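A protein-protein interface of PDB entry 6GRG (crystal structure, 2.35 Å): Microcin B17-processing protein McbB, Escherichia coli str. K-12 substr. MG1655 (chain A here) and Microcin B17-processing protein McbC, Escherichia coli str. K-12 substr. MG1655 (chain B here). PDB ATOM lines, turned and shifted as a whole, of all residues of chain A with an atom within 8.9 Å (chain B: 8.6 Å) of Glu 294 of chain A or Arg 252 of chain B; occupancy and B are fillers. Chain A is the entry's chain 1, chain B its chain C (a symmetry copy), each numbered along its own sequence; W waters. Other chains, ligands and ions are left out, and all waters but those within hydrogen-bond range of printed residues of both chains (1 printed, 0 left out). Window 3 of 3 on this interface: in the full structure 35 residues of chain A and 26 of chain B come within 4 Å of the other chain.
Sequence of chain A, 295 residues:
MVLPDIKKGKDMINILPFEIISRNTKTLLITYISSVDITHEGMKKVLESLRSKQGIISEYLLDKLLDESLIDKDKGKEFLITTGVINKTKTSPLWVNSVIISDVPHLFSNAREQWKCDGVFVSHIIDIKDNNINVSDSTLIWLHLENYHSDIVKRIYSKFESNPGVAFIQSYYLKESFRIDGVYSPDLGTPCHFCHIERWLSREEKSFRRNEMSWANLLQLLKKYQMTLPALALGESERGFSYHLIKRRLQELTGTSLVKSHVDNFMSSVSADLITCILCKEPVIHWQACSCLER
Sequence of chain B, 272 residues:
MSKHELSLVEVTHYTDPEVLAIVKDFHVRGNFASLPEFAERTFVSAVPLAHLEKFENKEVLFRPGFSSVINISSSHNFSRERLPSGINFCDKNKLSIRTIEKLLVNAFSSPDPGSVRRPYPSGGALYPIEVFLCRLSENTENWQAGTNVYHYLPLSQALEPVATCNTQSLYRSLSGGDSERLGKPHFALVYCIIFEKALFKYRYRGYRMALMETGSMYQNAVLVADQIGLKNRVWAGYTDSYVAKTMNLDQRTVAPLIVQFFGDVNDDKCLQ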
ATOM      1  N   GLU A 161       2.416 -17.490  13.799  1.00  0.00           N
ATOM      2  CA  GLU A 161       1.187 -17.867  13.034  1.00  0.00           C
ATOM      3  C   GLU A 161       0.605 -19.214  13.483  1.00  0.00           C
ATOM      4  O   GLU A 161      -0.616 -19.390  13.477  1.00  0.00           O
ATOM      5  CB  GLU A 161       1.447 -17.962  11.542  1.00  0.00           C
ATOM      6  CG  GLU A 161       1.183 -16.671  10.805  1.00  0.00           C
ATOM      7  CD  GLU A 161       1.419 -16.786   9.308  1.00  0.00           C
ATOM      8  OE1 GLU A 161       2.133 -17.753   8.891  1.00  0.00           O
ATOM      9  OE2 GLU A 161       0.894 -15.912   8.562  1.00  0.00           O
ATOM     10  N   TYR A 184      -5.733  -9.752  12.384  1.00  0.00           N
ATOM     11  CA  TYR A 184      -5.296 -10.857  11.586  1.00  0.00           C
ATOM     12  C   TYR A 184      -5.409 -12.115  12.446  1.00  0.00           C
ATOM     13  O   TYR A 184      -4.667 -12.263  13.422  1.00  0.00           O
ATOM     14  CB  TYR A 184      -3.873 -10.625  11.041  1.00  0.00           C
ATOM     15  CG  TYR A 184      -3.313 -11.854  10.372  1.00  0.00           C
ATOM     16  CD1 TYR A 184      -4.115 -12.622   9.542  1.00  0.00           C
ATOM     17  CD2 TYR A 184      -2.023 -12.303  10.609  1.00  0.00           C
ATOM     18  CE1 TYR A 184      -3.663 -13.798   8.972  1.00  0.00           C
ATOM     19  CE2 TYR A 184      -1.546 -13.474  10.033  1.00  0.00           C
ATOM     20  CZ  TYR A 184      -2.367 -14.221   9.200  1.00  0.00           C
ATOM     21  OH  TYR A 184      -1.930 -15.358   8.587  1.00  0.00           O
ATOM     22  N   GLY A 189      -9.850 -16.408   9.455  1.00  0.00           N
ATOM     23  CA  GLY A 189      -9.619 -16.273   8.006  1.00  0.00           C
ATOM     24  C   GLY A 189      -9.476 -14.835   7.547  1.00  0.00           C
ATOM     25  O   GLY A 189      -9.744 -14.539   6.394  1.00  0.00           O
ATOM     26  N   CYS A 195      -2.056  -7.704   3.315  1.00  0.00           N
ATOM     27  CA  CYS A 195      -3.329  -7.428   2.637  1.00  0.00           C
ATOM     28  C   CYS A 195      -3.659  -5.943   2.815  1.00  0.00           C
ATOM     29  O   CYS A 195      -4.165  -5.314   1.888  1.00  0.00           O
ATOM     30  CB  CYS A 195      -4.454  -8.328   3.134  1.00  0.00           C
ATOM     31  SG  CYS A 195      -4.324 -10.018   2.491  1.00  0.00           S
ATOM     32  N   ILE A 285     -10.177  -6.100   1.781  1.00  0.00           N
ATOM     33  CA  ILE A 285     -10.285  -7.435   1.139  1.00  0.00           C
ATOM     34  C   ILE A 285      -8.931  -8.171   1.195  1.00  0.00           C
ATOM     35  O   ILE A 285      -7.862  -7.586   1.371  1.00  0.00           O
ATOM     36  CB  ILE A 285     -10.784  -7.311  -0.312  1.00  0.00           C
ATOM     37  CG1 ILE A 285      -9.777  -6.591  -1.215  1.00  0.00           C
ATOM     38  CG2 ILE A 285     -12.147  -6.640  -0.350  1.00  0.00           C
ATOM     39  CD1 ILE A 285     -10.128  -6.616  -2.679  1.00  0.00           C
ATOM     40  N   HIS A 286      -8.973  -9.484   1.016  1.00  0.00           N
ATOM     41  CA  HIS A 286      -7.734 -10.218   0.825  1.00  0.00           C
ATOM     42  C   HIS A 286      -7.048  -9.704  -0.451  1.00  0.00           C
ATOM     43  O   HIS A 286      -7.717  -9.513  -1.489  1.00  0.00           O
ATOM     44  CB  HIS A 286      -8.027 -11.723   0.773  1.00  0.00           C
ATOM     45  CG  HIS A 286      -8.412 -12.326   2.086  1.00  0.00           C
ATOM     46  ND1 HIS A 286      -9.732 -12.549   2.436  1.00  0.00           N
ATOM     47  CD2 HIS A 286      -7.656 -12.766   3.121  1.00  0.00           C
ATOM     48  CE1 HIS A 286      -9.767 -13.105   3.635  1.00  0.00           C
ATOM     49  NE2 HIS A 286      -8.502 -13.259   4.071  1.00  0.00           N
ATOM     50  N   TRP A 287      -5.730  -9.470  -0.365  1.00  0.00           N
ATOM     51  CA  TRP A 287      -4.889  -9.167  -1.519  1.00  0.00           C
ATOM     52  C   TRP A 287      -4.660 -10.441  -2.349  1.00  0.00           C
ATOM     53  O   TRP A 287      -4.317 -11.501  -1.811  1.00  0.00           O
ATOM     54  CB  TRP A 287      -3.565  -8.550  -1.068  1.00  0.00           C
ATOM     55  CG  TRP A 287      -2.617  -8.192  -2.172  1.00  0.00           C
ATOM     56  CD1 TRP A 287      -2.916  -7.597  -3.362  1.00  0.00           C
ATOM     57  CD2 TRP A 287      -1.184  -8.352  -2.154  1.00  0.00           C
ATOM     58  NE1 TRP A 287      -1.771  -7.399  -4.096  1.00  0.00           N
ATOM     59  CE2 TRP A 287      -0.693  -7.843  -3.373  1.00  0.00           C
ATOM     60  CE3 TRP A 287      -0.272  -8.874  -1.223  1.00  0.00           C
ATOM     61  CZ2 TRP A 287       0.660  -7.859  -3.688  1.00  0.00           C
ATOM     62  CZ3 TRP A 287       1.072  -8.876  -1.530  1.00  0.00           C
ATOM     63  CH2 TRP A 287       1.527  -8.383  -2.755  1.00  0.00           C
ATOM     64  N   GLN A 288      -4.839 -10.320  -3.674  1.00  0.00           N
ATOM     65  CA  GLN A 288      -4.883 -11.474  -4.583  1.00  0.00           C
ATOM     66  C   GLN A 288      -3.525 -12.204  -4.608  1.00  0.00           C
ATOM     67  O   GLN A 288      -3.460 -13.402  -4.825  1.00  0.00           O
ATOM     68  CB  GLN A 288      -5.334 -11.018  -5.978  1.00  0.00           C
ATOM     69  CG  GLN A 288      -4.449  -9.954  -6.634  1.00  0.00           C
ATOM     70  CD  GLN A 288      -5.113  -9.306  -7.832  1.00  0.00           C
ATOM     71  OE1 GLN A 288      -6.130  -9.780  -8.371  1.00  0.00           O
ATOM     72  NE2 GLN A 288      -4.530  -8.199  -8.267  1.00  0.00           N
ATOM     73  N   ALA A 289      -2.436 -11.461  -4.408  1.00  0.00           N
ATOM     74  CA  ALA A 289      -1.128 -11.994  -4.539  1.00  0.00           C
ATOM     75  C   ALA A 289      -0.582 -12.414  -3.166  1.00  0.00           C
ATOM     76  O   ALA A 289       0.606 -12.729  -3.038  1.00  0.00           O
ATOM     77  CB  ALA A 289      -0.256 -10.959  -5.195  1.00  0.00           C
ATOM     78  N   CYS A 290      -1.452 -12.439  -2.144  1.00  0.00           N
ATOM     79  CA  CYS A 290      -1.019 -12.712  -0.801  1.00  0.00           C
ATOM     80  C   CYS A 290      -1.162 -14.191  -0.508  1.00  0.00           C
ATOM     81  O   CYS A 290      -1.983 -14.855  -1.103  1.00  0.00           O
ATOM     82  CB  CYS A 290      -1.844 -11.977   0.241  1.00  0.00           C
ATOM     83  SG  CYS A 290      -1.004 -11.787   1.832  1.00  0.00           S
ATOM     84  N   SER A 291      -0.404 -14.637   0.494  1.00  0.00           N
ATOM     85  CA  SER A 291      -0.259 -16.039   0.863  1.00  0.00           C
ATOM     86  C   SER A 291      -1.065 -16.401   2.124  1.00  0.00           C
ATOM     87  O   SER A 291      -1.169 -17.581   2.426  1.00  0.00           O
ATOM     88  CB  SER A 291       1.201 -16.345   1.089  1.00  0.00           C
ATOM     89  OG  SER A 291       1.661 -15.719   2.286  1.00  0.00           O
ATOM     90  N   CYS A 292      -1.614 -15.412   2.849  1.00  0.00           N
ATOM     91  CA  CYS A 292      -2.129 -15.639   4.206  1.00  0.00           C
ATOM     92  C   CYS A 292      -3.312 -16.625   4.201  1.00  0.00           C
ATOM     93  O   CYS A 292      -3.536 -17.310   5.181  1.00  0.00           O
ATOM     94  CB  CYS A 292      -2.473 -14.333   4.925  1.00  0.00           C
ATOM     95  SG  CYS A 292      -3.758 -13.313   4.146  1.00  0.00           S
ATOM     96  N   LEU A 293      -4.049 -16.721   3.092  1.00  0.00           N
ATOM     97  CA  LEU A 293      -5.163 -17.667   2.974  1.00  0.00           C
ATOM     98  C   LEU A 293      -4.681 -19.118   2.817  1.00  0.00           C
ATOM     99  O   LEU A 293      -5.433 -20.035   3.151  1.00  0.00           O
ATOM    100  CB  LEU A 293      -6.010 -17.318   1.750  1.00  0.00           C
ATOM    101  CG  LEU A 293      -6.699 -15.969   1.793  1.00  0.00           C
ATOM    102  CD1 LEU A 293      -6.084 -15.050   0.755  1.00  0.00           C
ATOM    103  CD2 LEU A 293      -8.183 -16.145   1.557  1.00  0.00           C
ATOM    104  N   GLU A 294      -3.489 -19.301   2.234  1.00  0.00           N
ATOM    105  CA  GLU A 294      -2.964 -20.610   1.883  1.00  0.00           C
ATOM    106  C   GLU A 294      -2.282 -21.259   3.095  1.00  0.00           C
ATOM    107  O   GLU A 294      -2.035 -22.438   3.092  1.00  0.00           O
ATOM    108  CB  GLU A 294      -1.921 -20.539   0.768  1.00  0.00           C
ATOM    109  CG  GLU A 294      -2.269 -19.627  -0.389  1.00  0.00           C
ATOM    110  CD  GLU A 294      -1.055 -19.367  -1.270  1.00  0.00           C
ATOM    111  OE1 GLU A 294      -0.169 -18.557  -0.878  1.00  0.00           O
ATOM    112  OE2 GLU A 294      -0.963 -20.021  -2.318  1.00  0.00           O
ATOM    113  N   ARG A 295      -1.938 -20.463   4.107  1.00  0.00           N
ATOM    114  CA  ARG A 295      -1.305 -20.986   5.320  1.00  0.00           C
ATOM    115  C   ARG A 295      -2.400 -21.687   6.145  1.00  0.00           C
ATOM    116  O   ARG A 295      -3.503 -21.183   6.323  1.00  0.00           O
ATOM    117  CB  ARG A 295      -0.485 -19.870   5.993  1.00  0.00           C
ATOM    118  CG  ARG A 295       0.786 -19.571   5.204  1.00  0.00           C
ATOM    119  CD  ARG A 295       1.817 -18.747   5.928  1.00  0.00           C
ATOM    120  NE  ARG A 295       1.409 -17.359   5.955  1.00  0.00           N
ATOM    121  CZ  ARG A 295       2.196 -16.324   5.658  1.00  0.00           C
ATOM    122  NH1 ARG A 295       3.420 -16.557   5.203  1.00  0.00           N
ATOM    123  NH2 ARG A 295       1.770 -15.076   5.863  1.00  0.00           N
ATOM    124  OXT ARG A 295      -2.260 -22.844   6.572  1.00  0.00           O
ATOM    125  N   LEU B  20     -13.854  -6.393 -10.342  1.00  0.00           N
ATOM    126  CA  LEU B  20     -13.721  -7.413  -9.338  1.00  0.00           C
ATOM    127  C   LEU B  20     -13.307  -6.798  -8.011  1.00  0.00           C
ATOM    128  O   LEU B  20     -13.801  -7.183  -6.967  1.00  0.00           O
ATOM    129  CB  LEU B  20     -12.665  -8.410  -9.809  1.00  0.00           C
ATOM    130  CG  LEU B  20     -12.411  -9.572  -8.858  1.00  0.00           C
ATOM    131  CD1 LEU B  20     -13.630 -10.491  -8.780  1.00  0.00           C
ATOM    132  CD2 LEU B  20     -11.177 -10.334  -9.288  1.00  0.00           C
ATOM    133  N   LYS B  24     -15.712  -6.642  -4.645  1.00  0.00           N
ATOM    134  CA  LYS B  24     -15.254  -7.294  -3.426  1.00  0.00           C
ATOM    135  C   LYS B  24     -15.136  -6.265  -2.296  1.00  0.00           C
ATOM    136  O   LYS B  24     -15.527  -6.563  -1.171  1.00  0.00           O
ATOM    137  CB  LYS B  24     -13.897  -7.971  -3.608  1.00  0.00           C
ATOM    138  CG  LYS B  24     -13.851  -9.224  -4.468  1.00  0.00           C
ATOM    139  CD  LYS B  24     -12.408  -9.474  -4.917  1.00  0.00           C
ATOM    140  CE  LYS B  24     -12.079 -10.913  -5.242  1.00  0.00           C
ATOM    141  NZ  LYS B  24     -10.701 -11.275  -4.804  1.00  0.00           N
ATOM    142  N   ILE B 193     -21.060 -17.311  -3.667  1.00  0.00           N
ATOM    143  CA  ILE B 193     -20.858 -16.657  -4.934  1.00  0.00           C
ATOM    144  C   ILE B 193     -19.409 -16.903  -5.354  1.00  0.00           C
ATOM    145  O   ILE B 193     -18.531 -16.732  -4.546  1.00  0.00           O
ATOM    146  CB  ILE B 193     -21.177 -15.150  -4.818  1.00  0.00           C
ATOM    147  CG1 ILE B 193     -21.200 -14.506  -6.199  1.00  0.00           C
ATOM    148  CG2 ILE B 193     -20.210 -14.414  -3.895  1.00  0.00           C
ATOM    149  CD1 ILE B 193     -21.649 -13.095  -6.200  1.00  0.00           C
ATOM    150  N   ILE B 194     -19.184 -17.296  -6.613  1.00  0.00           N
ATOM    151  CA  ILE B 194     -17.857 -17.244  -7.244  1.00  0.00           C
ATOM    152  C   ILE B 194     -17.747 -15.910  -7.995  1.00  0.00           C
ATOM    153  O   ILE B 194     -18.371 -15.718  -9.043  1.00  0.00           O
ATOM    154  CB  ILE B 194     -17.648 -18.439  -8.182  1.00  0.00           C
ATOM    155  CG1 ILE B 194     -17.880 -19.754  -7.449  1.00  0.00           C
ATOM    156  CG2 ILE B 194     -16.268 -18.394  -8.843  1.00  0.00           C
ATOM    157  CD1 ILE B 194     -17.738 -20.956  -8.356  1.00  0.00           C
ATOM    158  N   PHE B 195     -16.976 -14.975  -7.435  1.00  0.00           N
ATOM    159  CA  PHE B 195     -17.049 -13.584  -7.854  1.00  0.00           C
ATOM    160  C   PHE B 195     -16.847 -13.447  -9.374  1.00  0.00           C
ATOM    161  O   PHE B 195     -17.671 -12.842 -10.040  1.00  0.00           O
ATOM    162  CB  PHE B 195     -16.019 -12.742  -7.099  1.00  0.00           C
ATOM    163  CG  PHE B 195     -16.292 -12.560  -5.632  1.00  0.00           C
ATOM    164  CD1 PHE B 195     -17.385 -11.830  -5.202  1.00  0.00           C
ATOM    165  CD2 PHE B 195     -15.423 -13.072  -4.676  1.00  0.00           C
ATOM    166  CE1 PHE B 195     -17.619 -11.633  -3.847  1.00  0.00           C
ATOM    167  CE2 PHE B 195     -15.665 -12.895  -3.321  1.00  0.00           C
ATOM    168  CZ  PHE B 195     -16.769 -12.179  -2.911  1.00  0.00           C
ATOM    169  N   GLU B 196     -15.781 -14.037  -9.923  1.00  0.00           N
ATOM    170  CA  GLU B 196     -15.431 -13.840 -11.350  1.00  0.00           C
ATOM    171  C   GLU B 196     -16.518 -14.430 -12.264  1.00  0.00           C
ATOM    172  O   GLU B 196     -16.808 -13.907 -13.346  1.00  0.00           O
ATOM    173  CB  GLU B 196     -14.016 -14.367 -11.623  1.00  0.00           C
ATOM    174  CG  GLU B 196     -12.916 -13.494 -11.008  1.00  0.00           C
ATOM    175  CD  GLU B 196     -11.498 -13.715 -11.527  1.00  0.00           C
ATOM    176  OE1 GLU B 196     -11.320 -13.734 -12.772  1.00  0.00           O
ATOM    177  OE2 GLU B 196     -10.552 -13.872 -10.676  1.00  0.00           O
ATOM    178  N   ALA B 244     -16.017 -19.631   5.541  1.00  0.00           N
ATOM    179  CA  ALA B 244     -15.110 -19.796   4.414  1.00  0.00           C
ATOM    180  C   ALA B 244     -13.898 -20.618   4.834  1.00  0.00           C
ATOM    181  O   ALA B 244     -13.571 -21.578   4.181  1.00  0.00           O
ATOM    182  CB  ALA B 244     -14.667 -18.462   3.885  1.00  0.00           C
ATOM    183  N   LYS B 245     -13.251 -20.225   5.928  1.00  0.00           N
ATOM    184  CA  LYS B 245     -11.989 -20.844   6.354  1.00  0.00           C
ATOM    185  C   LYS B 245     -12.223 -22.331   6.644  1.00  0.00           C
ATOM    186  O   LYS B 245     -11.394 -23.191   6.271  1.00  0.00           O
ATOM    187  CB  LYS B 245     -11.443 -20.138   7.598  1.00  0.00           C
ATOM    188  CG  LYS B 245     -10.281 -20.831   8.305  1.00  0.00           C
ATOM    189  CD  LYS B 245      -8.931 -20.433   7.770  1.00  0.00           C
ATOM    190  CE  LYS B 245      -7.838 -21.299   8.365  1.00  0.00           C
ATOM    191  NZ  LYS B 245      -6.544 -20.574   8.430  1.00  0.00           N
ATOM    192  N   ASN B 248     -12.764 -24.601   3.845  1.00  0.00           N
ATOM    193  CA  ASN B 248     -11.566 -24.595   3.005  1.00  0.00           C
ATOM    194  C   ASN B 248     -11.843 -23.912   1.650  1.00  0.00           C
ATOM    195  O   ASN B 248     -11.208 -24.206   0.662  1.00  0.00           O
ATOM    196  CB  ASN B 248     -10.970 -26.007   2.895  1.00  0.00           C
ATOM    197  CG  ASN B 248     -10.233 -26.465   4.143  1.00  0.00           C
ATOM    198  OD1 ASN B 248      -9.431 -25.740   4.717  1.00  0.00           O
ATOM    199  ND2 ASN B 248     -10.469 -27.694   4.558  1.00  0.00           N
ATOM    200  N   LEU B 249     -12.762 -22.952   1.624  1.00  0.00           N
ATOM    201  CA  LEU B 249     -12.949 -22.061   0.477  1.00  0.00           C
ATOM    202  C   LEU B 249     -11.834 -21.005   0.476  1.00  0.00           C
ATOM    203  O   LEU B 249     -11.390 -20.564   1.505  1.00  0.00           O
ATOM    204  CB  LEU B 249     -14.314 -21.371   0.554  1.00  0.00           C
ATOM    205  CG  LEU B 249     -15.542 -22.265   0.757  1.00  0.00           C
ATOM    206  CD1 LEU B 249     -16.798 -21.410   0.857  1.00  0.00           C
ATOM    207  CD2 LEU B 249     -15.704 -23.290  -0.351  1.00  0.00           C
ATOM    208  N   ASP B 250     -11.381 -20.639  -0.719  1.00  0.00           N
ATOM    209  CA  ASP B 250     -10.471 -19.573  -0.933  1.00  0.00           C
ATOM    210  C   ASP B 250     -11.301 -18.299  -1.130  1.00  0.00           C
ATOM    211  O   ASP B 250     -12.012 -18.148  -2.129  1.00  0.00           O
ATOM    212  CB  ASP B 250      -9.600 -19.890  -2.141  1.00  0.00           C
ATOM    213  CG  ASP B 250      -8.482 -18.893  -2.395  1.00  0.00           C
ATOM    214  OD1 ASP B 250      -8.529 -17.772  -1.824  1.00  0.00           O
ATOM    215  OD2 ASP B 250      -7.567 -19.242  -3.175  1.00  0.00           O
ATOM    216  N   GLN B 251     -11.184 -17.368  -0.175  1.00  0.00           N
ATOM    217  CA  GLN B 251     -12.011 -16.157  -0.136  1.00  0.00           C
ATOM    218  C   GLN B 251     -11.687 -15.188  -1.291  1.00  0.00           C
ATOM    219  O   GLN B 251     -12.452 -14.277  -1.527  1.00  0.00           O
ATOM    220  CB  GLN B 251     -11.841 -15.441   1.210  1.00  0.00           C
ATOM    221  CG  GLN B 251     -12.106 -16.338   2.411  1.00  0.00           C
ATOM    222  CD  GLN B 251     -12.101 -15.553   3.700  1.00  0.00           C
ATOM    223  OE1 GLN B 251     -12.747 -14.519   3.808  1.00  0.00           O
ATOM    224  NE2 GLN B 251     -11.366 -16.038   4.687  1.00  0.00           N
ATOM    225  N   ARG B 252     -10.537 -15.326  -1.964  1.00  0.00           N
ATOM    226  CA  ARG B 252     -10.222 -14.487  -3.124  1.00  0.00           C
ATOM    227  C   ARG B 252     -11.139 -14.832  -4.314  1.00  0.00           C
ATOM    228  O   ARG B 252     -11.360 -13.991  -5.187  1.00  0.00           O
ATOM    229  CB  ARG B 252      -8.758 -14.664  -3.533  1.00  0.00           C
ATOM    230  CG  ARG B 252      -7.749 -14.097  -2.546  1.00  0.00           C
ATOM    231  CD  ARG B 252      -6.327 -14.598  -2.755  1.00  0.00           C
ATOM    232  NE  ARG B 252      -6.232 -16.041  -2.581  1.00  0.00           N
ATOM    233  CZ  ARG B 252      -5.136 -16.749  -2.793  1.00  0.00           C
ATOM    234  NH1 ARG B 252      -4.036 -16.142  -3.191  1.00  0.00           N
ATOM    235  NH2 ARG B 252      -5.125 -18.048  -2.556  1.00  0.00           N
ATOM    236  N   THR B 253     -11.694 -16.054  -4.331  1.00  0.00           N
ATOM    237  CA  THR B 253     -12.490 -16.554  -5.452  1.00  0.00           C
ATOM    238  C   THR B 253     -13.979 -16.666  -5.116  1.00  0.00           C
ATOM    239  O   THR B 253     -14.844 -16.438  -5.997  1.00  0.00           O
ATOM    240  CB  THR B 253     -11.957 -17.934  -5.854  1.00  0.00           C
ATOM    241  OG1 THR B 253     -10.682 -17.690  -6.441  1.00  0.00           O
ATOM    242  CG2 THR B 253     -12.850 -18.705  -6.798  1.00  0.00           C
ATOM    243  N   VAL B 254     -14.270 -17.075  -3.876  1.00  0.00           N
ATOM    244  CA  VAL B 254     -15.606 -17.511  -3.495  1.00  0.00           C
ATOM    245  C   VAL B 254     -15.899 -17.065  -2.059  1.00  0.00           C
ATOM    246  O   VAL B 254     -15.024 -17.079  -1.238  1.00  0.00           O
ATOM    247  CB  VAL B 254     -15.760 -19.039  -3.642  1.00  0.00           C
ATOM    248  CG1 VAL B 254     -14.678 -19.828  -2.900  1.00  0.00           C
ATOM    249  CG2 VAL B 254     -17.139 -19.516  -3.216  1.00  0.00           C
ATOM    250  N   ALA B 255     -17.161 -16.716  -1.778  1.00  0.00           N
ATOM    251  CA  ALA B 255     -17.582 -16.228  -0.487  1.00  0.00           C
ATOM    252  C   ALA B 255     -18.980 -16.747  -0.169  1.00  0.00           C
ATOM    253  O   ALA B 255     -19.838 -16.789  -1.048  1.00  0.00           O
ATOM    254  CB  ALA B 255     -17.559 -14.715  -0.457  1.00  0.00           C
HETATM  255  O   HOH W   1      -9.781 -10.983  -2.420  1.00  0.00           O
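Lys 24 of chain B touches Ile 285 of chain A (O to CG2, 3.5 Å).
CE1 of His 286 of chain A touches OE1 of Gln 251 of chain B, at 3.3 Å.
Arg 252 of chain B touches Trp 287 of chain A.
Leu 293 of chain A touches Asp 250 of chain B.
Leu 293 of chain A touches Gln 251 of chain B.
Leu 293 of chain A touches Arg 252 of chain B.
NH2 of Arg 252 of chain B touches CG of Glu 294 of chain A, 3.9 Å away.
The backbone carbonyl oxygen of Gly 189 of chain A is in hydrogen-bond range of the side-chain amide nitrogen of Gln 251 of chain B.
O of Arg 295 of chain A lies within salt-bridge range of NZ of Lys 245 of chain B (3.7 Å).
The backbone carbonyl oxygen (O) of Gln 288 of chain A lies within hydrogen-bond range of the guanidinium group (NH1) of Arg 252 of chain B, 3.2 Å away.
The backbone carbonyl oxygen (O) of Cys 290 of chain A is in hydrogen-bond range of the guanidinium group (NH1) of Arg 252 of chain B, 3.2 Å away.
Of the 16 printed residues of chain B, 5 touch a printed residue of chain A.
Of the 15 printed residues of chain A, 9 touch a printed residue of chain B.
Hydrophobic or aromatic side chains of chain A that line the printed part of chain B: Ile 285, His 286 and Leu 293.
Among the printed residues, 11 pairs touch across the chains.
Among the printed residues, no Asp or Glu carboxylate lies within 4 Å of a Lys or Arg side-chain nitrogen of the other chain.
The backbone carbonyl oxygen of Arg 252 of chain B is in hydrogen-bond range of the side-chain amino group of Lys 24 of chain B (2.8 Å).
OD2 of Asp 250 of chain B is in salt-bridge range of NH2 of Arg 252 of chain B (2.8 Å).
NE2 of His 286 of chain A sits at hydrogen-bond distance from O of Gly 189 of chain A (2.9 Å).
OE2 of Glu 161 of chain A is in salt-bridge range of NH2 of Arg 295 of chain A (3.0 Å).
SG of Cys 195 of chain A sits close to N of Trp 287 of chain A (3.2 Å).
Water W1 bridges the side-chain amino group of Lys 24 of chain B (2.6 Å) and the backbone carbonyl oxygen of His 286 of chain A (2.7 Å).
Tyr 184 of chain A touches none of the printed residues of chain B.
Of the printed residues of chain B, Gly 189 of chain A touches Gln 251 (2.8 Å).
Of the printed residues of chain B, His 286 of chain A touches Gln 251.
Of chain B, only Asp 250 (3.8 Å), Gln 251 (3.7 Å) and Arg 252 (3.5 Å) come within 4 Å of Leu 293 of chain A.
Of chain B, only Arg 252 (3.9 Å) comes within 4 Å of Glu 294 of chain A.
Leu 249 of chain B touches none of the printed residues of chain A.
Of chain A, only Trp 287 (3.8 Å), Gln 288 (3.2 Å), Cys 290 (3.2 Å), Leu 293 (3.5 Å) and Glu 294 (3.9 Å) come within 4 Å of Arg 252 of chain B.
The nearest residue of chain B that does not touch Glu 294 of chain A is Asp 250 of chain B (6.0 Å).
The nearest residue of chain A that does not touch Arg 252 of chain B is His 286 of chain A (4.1 Å).
The nearest printed residue of chain A that does not touch Lys 245 of chain B is Gly 189 of chain A (4.2 Å).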
